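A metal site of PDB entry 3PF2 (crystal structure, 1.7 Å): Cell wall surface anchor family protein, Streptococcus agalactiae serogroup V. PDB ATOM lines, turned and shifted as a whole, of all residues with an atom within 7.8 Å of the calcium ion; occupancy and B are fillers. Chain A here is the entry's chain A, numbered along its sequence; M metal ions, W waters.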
ATOM      1  N   THR A   9      -9.394 -24.717  24.656  1.00  0.00           N
ATOM      2  CA  THR A   9     -10.232 -25.911  24.622  1.00  0.00           C
ATOM      3  C   THR A   9     -11.220 -25.920  25.780  1.00  0.00           C
ATOM      4  O   THR A   9     -10.983 -25.316  26.808  1.00  0.00           O
ATOM      5  CB  THR A   9      -9.396 -27.208  24.638  1.00  0.00           C
ATOM      6  OG1 THR A   9      -8.380 -27.120  25.646  1.00  0.00           O
ATOM      7  CG2 THR A   9      -8.732 -27.419  23.265  1.00  0.00           C
ATOM      8  N   ASP A  10     -12.336 -26.613  25.582  1.00  0.00           N
ATOM      9  CA  ASP A  10     -13.325 -26.806  26.647  1.00  0.00           C
ATOM     10  C   ASP A  10     -14.085 -28.076  26.330  1.00  0.00           C
ATOM     11  O   ASP A  10     -14.079 -28.541  25.193  1.00  0.00           O
ATOM     12  CB  ASP A  10     -14.309 -25.622  26.687  1.00  0.00           C
ATOM     13  CG  ASP A  10     -15.420 -25.816  27.718  1.00  0.00           C
ATOM     14  OD1 ASP A  10     -15.146 -26.312  28.820  1.00  0.00           O
ATOM     15  OD2 ASP A  10     -16.573 -25.463  27.446  1.00  0.00           O
ATOM     16  N   LYS A  11     -14.755 -28.640  27.331  1.00  0.00           N
ATOM     17  CA  LYS A  11     -15.622 -29.792  27.090  1.00  0.00           C
ATOM     18  C   LYS A  11     -16.965 -29.502  27.774  1.00  0.00           C
ATOM     19  O   LYS A  11     -17.008 -28.935  28.859  1.00  0.00           O
ATOM     20  CB  LYS A  11     -14.976 -31.065  27.646  1.00  0.00           C
ATOM     21  CG  LYS A  11     -15.630 -32.393  27.207  1.00  0.00           C
ATOM     22  CD  LYS A  11     -14.929 -33.594  27.858  1.00  0.00           C
ATOM     23  CE  LYS A  11     -15.558 -34.923  27.420  1.00  0.00           C
ATOM     24  NZ  LYS A  11     -14.748 -36.099  27.859  1.00  0.00           N
ATOM     25  N   ASP A  12     -18.053 -29.892  27.110  1.00  0.00           N
ATOM     26  CA  ASP A  12     -19.405 -29.805  27.661  1.00  0.00           C
ATOM     27  C   ASP A  12     -20.046 -31.193  27.644  1.00  0.00           C
ATOM     28  O   ASP A  12     -19.489 -32.147  27.108  1.00  0.00           O
ATOM     29  CB  ASP A  12     -20.281 -28.893  26.788  1.00  0.00           C
ATOM     30  CG  ASP A  12     -19.845 -27.429  26.827  1.00  0.00           C
ATOM     31  OD1 ASP A  12     -18.994 -27.059  27.692  1.00  0.00           O
ATOM     32  OD2 ASP A  12     -20.330 -26.666  25.973  1.00  0.00           O
ATOM     33  N   VAL A  13     -21.222 -31.293  28.253  1.00  0.00           N
ATOM     34  CA  VAL A  13     -22.020 -32.511  28.202  1.00  0.00           C
ATOM     35  C   VAL A  13     -23.466 -32.142  27.959  1.00  0.00           C
ATOM     36  O   VAL A  13     -23.928 -31.062  28.363  1.00  0.00           O
ATOM     37  CB  VAL A  13     -21.882 -33.335  29.502  1.00  0.00           C
ATOM     38  CG1 VAL A  13     -22.558 -32.620  30.694  1.00  0.00           C
ATOM     39  CG2 VAL A  13     -22.395 -34.762  29.300  1.00  0.00           C
ATOM     40  N   LYS A  15     -25.502 -30.836  25.901  1.00  0.00           N
ATOM     41  CA  LYS A  15     -25.618 -29.893  24.806  1.00  0.00           C
ATOM     42  C   LYS A  15     -24.557 -28.827  24.987  1.00  0.00           C
ATOM     43  O   LYS A  15     -23.965 -28.686  26.068  1.00  0.00           O
ATOM     44  CB  LYS A  15     -27.008 -29.234  24.816  1.00  0.00           C
ATOM     45  CG  LYS A  15     -27.254 -28.358  26.047  1.00  0.00           C
ATOM     46  CD  LYS A  15     -28.732 -28.034  26.222  1.00  0.00           C
ATOM     47  CE  LYS A  15     -28.933 -26.974  27.299  1.00  0.00           C
ATOM     48  NZ  LYS A  15     -30.398 -26.893  27.670  1.00  0.00           N
ATOM     49  N   LEU A  16     -24.352 -28.033  23.943  1.00  0.00           N
ATOM     50  CA  LEU A  16     -23.415 -26.907  24.045  1.00  0.00           C
ATOM     51  C   LEU A  16     -23.856 -25.936  25.129  1.00  0.00           C
ATOM     52  O   LEU A  16     -25.013 -25.490  25.163  1.00  0.00           O
ATOM     53  CB  LEU A  16     -23.274 -26.171  22.713  1.00  0.00           C
ATOM     54  CG  LEU A  16     -22.532 -26.964  21.636  1.00  0.00           C
ATOM     55  CD1 LEU A  16     -22.615 -26.211  20.303  1.00  0.00           C
ATOM     56  CD2 LEU A  16     -21.070 -27.167  22.043  1.00  0.00           C
ATOM     57  N   GLY A  17     -22.918 -25.644  26.024  1.00  0.00           N
ATOM     58  CA  GLY A  17     -23.130 -24.673  27.086  1.00  0.00           C
ATOM     59  C   GLY A  17     -23.480 -25.299  28.418  1.00  0.00           C
ATOM     60  O   GLY A  17     -23.590 -24.584  29.430  1.00  0.00           O
ATOM     61  N   GLN A  18     -23.629 -26.622  28.448  1.00  0.00           N
ATOM     62  CA  GLN A  18     -24.008 -27.313  29.696  1.00  0.00           C
ATOM     63  C   GLN A  18     -22.822 -28.128  30.215  1.00  0.00           C
ATOM     64  O   GLN A  18     -22.128 -28.779  29.428  1.00  0.00           O
ATOM     65  CB  GLN A  18     -25.230 -28.209  29.472  1.00  0.00           C
ATOM     66  CG  GLN A  18     -25.714 -28.939  30.767  1.00  0.00           C
ATOM     67  CD  GLN A  18     -27.173 -29.439  30.735  1.00  0.00           C
ATOM     68  OE1 GLN A  18     -27.633 -30.094  31.680  1.00  0.00           O
ATOM     69  NE2 GLN A  18     -27.889 -29.164  29.665  1.00  0.00           N
ATOM     70  N   ASP A  19     -22.593 -28.099  31.543  1.00  0.00           N
ATOM     71  CA  ASP A  19     -21.444 -28.776  32.129  1.00  0.00           C
ATOM     72  C   ASP A  19     -21.778 -29.880  33.138  1.00  0.00           C
ATOM     73  O   ASP A  19     -20.881 -30.551  33.648  1.00  0.00           O
ATOM     74  CB  ASP A  19     -20.522 -27.744  32.796  1.00  0.00           C
ATOM     75  CG  ASP A  19     -19.854 -26.808  31.787  1.00  0.00           C
ATOM     76  OD1 ASP A  19     -19.252 -27.328  30.830  1.00  0.00           O
ATOM     77  OD2 ASP A  19     -19.963 -25.553  31.936  1.00  0.00           O
ATOM     78  N   ASP A  20     -23.076 -30.078  33.422  1.00  0.00           N
ATOM     79  CA  ASP A  20     -23.470 -31.046  34.443  1.00  0.00           C
ATOM     80  C   ASP A  20     -24.770 -31.682  34.029  1.00  0.00           C
ATOM     81  O   ASP A  20     -25.709 -30.983  33.646  1.00  0.00           O
ATOM     82  CB  ASP A  20     -23.703 -30.323  35.781  1.00  0.00           C
ATOM     83  CG  ASP A  20     -22.434 -29.698  36.329  1.00  0.00           C
ATOM     84  OD1 ASP A  20     -21.654 -30.408  36.988  1.00  0.00           O
ATOM     85  OD2 ASP A  20     -22.252 -28.463  36.113  1.00  0.00           O
ATOM     86  N   PHE A  32     -19.233 -32.956  24.356  1.00  0.00           N
ATOM     87  CA  PHE A  32     -18.811 -32.074  23.248  1.00  0.00           C
ATOM     88  C   PHE A  32     -17.380 -31.596  23.489  1.00  0.00           C
ATOM     89  O   PHE A  32     -17.134 -30.879  24.445  1.00  0.00           O
ATOM     90  CB  PHE A  32     -19.748 -30.876  23.114  1.00  0.00           C
ATOM     91  CG  PHE A  32     -21.150 -31.257  22.749  1.00  0.00           C
ATOM     92  CD1 PHE A  32     -21.569 -31.235  21.426  1.00  0.00           C
ATOM     93  CD2 PHE A  32     -22.035 -31.689  23.732  1.00  0.00           C
ATOM     94  CE1 PHE A  32     -22.890 -31.630  21.092  1.00  0.00           C
ATOM     95  CE2 PHE A  32     -23.345 -32.093  23.414  1.00  0.00           C
ATOM     96  CZ  PHE A  32     -23.776 -32.053  22.085  1.00  0.00           C
ATOM     97  N   LYS A  34     -14.470 -29.278  22.436  1.00  0.00           N
ATOM     98  CA  LYS A  34     -14.558 -27.979  21.791  1.00  0.00           C
ATOM     99  C   LYS A  34     -13.191 -27.336  21.718  1.00  0.00           C
ATOM    100  O   LYS A  34     -12.473 -27.356  22.693  1.00  0.00           O
ATOM    101  CB  LYS A  34     -15.483 -27.042  22.584  1.00  0.00           C
ATOM    102  CG  LYS A  34     -16.895 -27.609  22.828  1.00  0.00           C
ATOM    103  CD  LYS A  34     -17.505 -27.048  24.136  1.00  0.00           C
ATOM    104  CE  LYS A  34     -17.765 -25.524  24.050  1.00  0.00           C
ATOM    105  NZ  LYS A  34     -18.346 -24.979  25.325  1.00  0.00           N
ATOM    106  N   GLN A 116     -11.293 -17.962  25.727  1.00  0.00           N
ATOM    107  CA  GLN A 116     -11.635 -19.137  26.534  1.00  0.00           C
ATOM    108  C   GLN A 116     -13.044 -19.023  27.120  1.00  0.00           C
ATOM    109  O   GLN A 116     -13.789 -19.992  27.084  1.00  0.00           O
ATOM    110  CB  GLN A 116     -10.631 -19.326  27.673  1.00  0.00           C
ATOM    111  CG  GLN A 116     -10.978 -20.463  28.646  1.00  0.00           C
ATOM    112  CD  GLN A 116     -10.631 -21.827  28.080  1.00  0.00           C
ATOM    113  OE1 GLN A 116      -9.460 -22.108  27.797  1.00  0.00           O
ATOM    114  NE2 GLN A 116     -11.635 -22.675  27.913  1.00  0.00           N
ATOM    115  N   LEU A 119     -15.709 -19.420  24.567  1.00  0.00           N
ATOM    116  CA  LEU A 119     -15.783 -20.825  24.195  1.00  0.00           C
ATOM    117  C   LEU A 119     -16.612 -21.592  25.237  1.00  0.00           C
ATOM    118  O   LEU A 119     -17.540 -22.334  24.872  1.00  0.00           O
ATOM    119  CB  LEU A 119     -14.393 -21.446  24.011  1.00  0.00           C
ATOM    120  CG  LEU A 119     -14.438 -22.900  23.541  1.00  0.00           C
ATOM    121  CD1 LEU A 119     -15.009 -23.033  22.112  1.00  0.00           C
ATOM    122  CD2 LEU A 119     -13.066 -23.576  23.659  1.00  0.00           C
ATOM    123  N   ASP A 120     -16.297 -21.344  26.512  1.00  0.00           N
ATOM    124  CA  ASP A 120     -16.964 -22.025  27.634  1.00  0.00           C
ATOM    125  C   ASP A 120     -18.458 -21.756  27.632  1.00  0.00           C
ATOM    126  O   ASP A 120     -19.254 -22.611  28.062  1.00  0.00           O
ATOM    127  CB  ASP A 120     -16.416 -21.517  28.988  1.00  0.00           C
ATOM    128  CG  ASP A 120     -14.984 -21.930  29.260  1.00  0.00           C
ATOM    129  OD1 ASP A 120     -14.420 -22.762  28.522  1.00  0.00           O
ATOM    130  OD2 ASP A 120     -14.415 -21.433  30.245  1.00  0.00           O
ATOM    131  N   LYS A 121     -18.843 -20.555  27.183  1.00  0.00           N
ATOM    132  CA  LYS A 121     -20.229 -20.100  27.250  1.00  0.00           C
ATOM    133  C   LYS A 121     -20.990 -20.368  25.972  1.00  0.00           C
ATOM    134  O   LYS A 121     -22.180 -20.073  25.903  1.00  0.00           O
ATOM    135  CB  LYS A 121     -20.290 -18.599  27.558  1.00  0.00           C
ATOM    136  CG  LYS A 121     -20.550 -18.246  29.025  1.00  0.00           C
ATOM    137  CD  LYS A 121     -19.380 -18.596  29.878  1.00  0.00           C
ATOM    138  CE  LYS A 121     -19.581 -18.183  31.329  1.00  0.00           C
ATOM    139  NZ  LYS A 121     -18.344 -18.408  32.117  1.00  0.00           N
ATOM    140  N   ALA A 122     -20.330 -20.910  24.958  1.00  0.00           N
ATOM    141  CA  ALA A 122     -20.950 -21.113  23.639  1.00  0.00           C
ATOM    142  C   ALA A 122     -22.133 -22.075  23.727  1.00  0.00           C
ATOM    143  O   ALA A 122     -22.019 -23.158  24.313  1.00  0.00           O
ATOM    144  CB  ALA A 122     -19.929 -21.614  22.620  1.00  0.00           C
ATOM    145  N   PRO A 173      -8.888 -28.143  28.614  1.00  0.00           N
ATOM    146  CA  PRO A 173      -9.981 -27.407  29.267  1.00  0.00           C
ATOM    147  C   PRO A 173      -9.643 -27.013  30.725  1.00  0.00           C
ATOM    148  O   PRO A 173      -9.147 -27.848  31.500  1.00  0.00           O
ATOM    149  CB  PRO A 173     -11.140 -28.405  29.236  1.00  0.00           C
ATOM    150  CG  PRO A 173     -10.853 -29.281  28.042  1.00  0.00           C
ATOM    151  CD  PRO A 173      -9.340 -29.450  28.088  1.00  0.00           C
ATOM    152  N   ARG A 175     -11.822 -26.225  33.003  1.00  0.00           N
ATOM    153  CA  ARG A 175     -12.901 -26.749  33.853  1.00  0.00           C
ATOM    154  C   ARG A 175     -13.530 -27.937  33.139  1.00  0.00           C
ATOM    155  O   ARG A 175     -13.733 -27.873  31.917  1.00  0.00           O
ATOM    156  CB  ARG A 175     -13.945 -25.671  34.128  1.00  0.00           C
ATOM    157  CG  ARG A 175     -13.429 -24.510  34.989  1.00  0.00           C
ATOM    158  CD  ARG A 175     -14.222 -23.228  34.759  1.00  0.00           C
ATOM    159  NE  ARG A 175     -13.863 -22.545  33.508  1.00  0.00           N
ATOM    160  CZ  ARG A 175     -12.832 -21.724  33.358  1.00  0.00           C
ATOM    161  NH1 ARG A 175     -12.026 -21.440  34.376  1.00  0.00           N
ATOM    162  NH2 ARG A 175     -12.604 -21.160  32.168  1.00  0.00           N
ATOM    163  N   LYS A 176     -13.811 -28.994  33.917  1.00  0.00           N
ATOM    164  CA  LYS A 176     -14.283 -30.291  33.410  1.00  0.00           C
ATOM    165  C   LYS A 176     -15.798 -30.425  33.623  1.00  0.00           C
ATOM    166  O   LYS A 176     -16.308 -30.128  34.709  1.00  0.00           O
ATOM    167  CB  LYS A 176     -13.589 -31.439  34.128  1.00  0.00           C
ATOM    168  CG  LYS A 176     -12.061 -31.476  34.001  1.00  0.00           C
ATOM    169  CD  LYS A 176     -11.531 -32.818  34.544  1.00  0.00           C
ATOM    170  CE  LYS A 176      -9.997 -32.812  34.718  1.00  0.00           C
ATOM    171  NZ  LYS A 176      -9.515 -34.201  35.021  1.00  0.00           N
ATOM    172  N   PRO A 177     -16.527 -30.869  32.576  1.00  0.00           N
ATOM    173  CA  PRO A 177     -17.933 -31.263  32.780  1.00  0.00           C
ATOM    174  C   PRO A 177     -18.039 -32.617  33.467  1.00  0.00           C
ATOM    175  O   PRO A 177     -17.053 -33.357  33.536  1.00  0.00           O
ATOM    176  CB  PRO A 177     -18.489 -31.325  31.354  1.00  0.00           C
ATOM    177  CG  PRO A 177     -17.291 -31.727  30.517  1.00  0.00           C
ATOM    178  CD  PRO A 177     -16.087 -31.060  31.179  1.00  0.00           C
HETATM  179 CA    CA M   1     -17.568 -26.691  29.388  1.00  0.00          CA
HETATM  180  O   HOH W   1     -18.350 -24.521  30.014  1.00  0.00           O
HETATM  181  O   HOH W   2     -16.475 -27.022  31.462  1.00  0.00           O
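OD2 of Asp 12 is in salt-bridge range of NZ of Lys 34 (2.7 Å).
OD2 of Asp 12 lies within hydrogen-bond range of N of Gly 17.
O of Asp 12 sits at hydrogen-bond distance from N of Phe 32 (2.9 Å).
O of Asp 10 sits at hydrogen-bond distance from N of Lys 34 (2.9 Å).
Four residues have an atom within 4 Å of the calcium ion: Asp 10, Lys 11, Asp 12 and Asp 19.
The calcium ion is bound by OD1 of Asp 12 (2.2 Å), OD1 of Asp 19 (2.3 Å), water W2 (2.4 Å), O of Lys 11 (2.4 Å), water W1 (2.4 Å), OD2 of Asp 10 (2.5 Å) and OD1 of Asp 10 (2.5 Å).
Water W1 lies within hydrogen-bond range of the side-chain carboxylate (OD2) of Asp 19 (2.7 Å) and the backbone carbonyl oxygen (O) of Asp 120 (2.9 Å).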
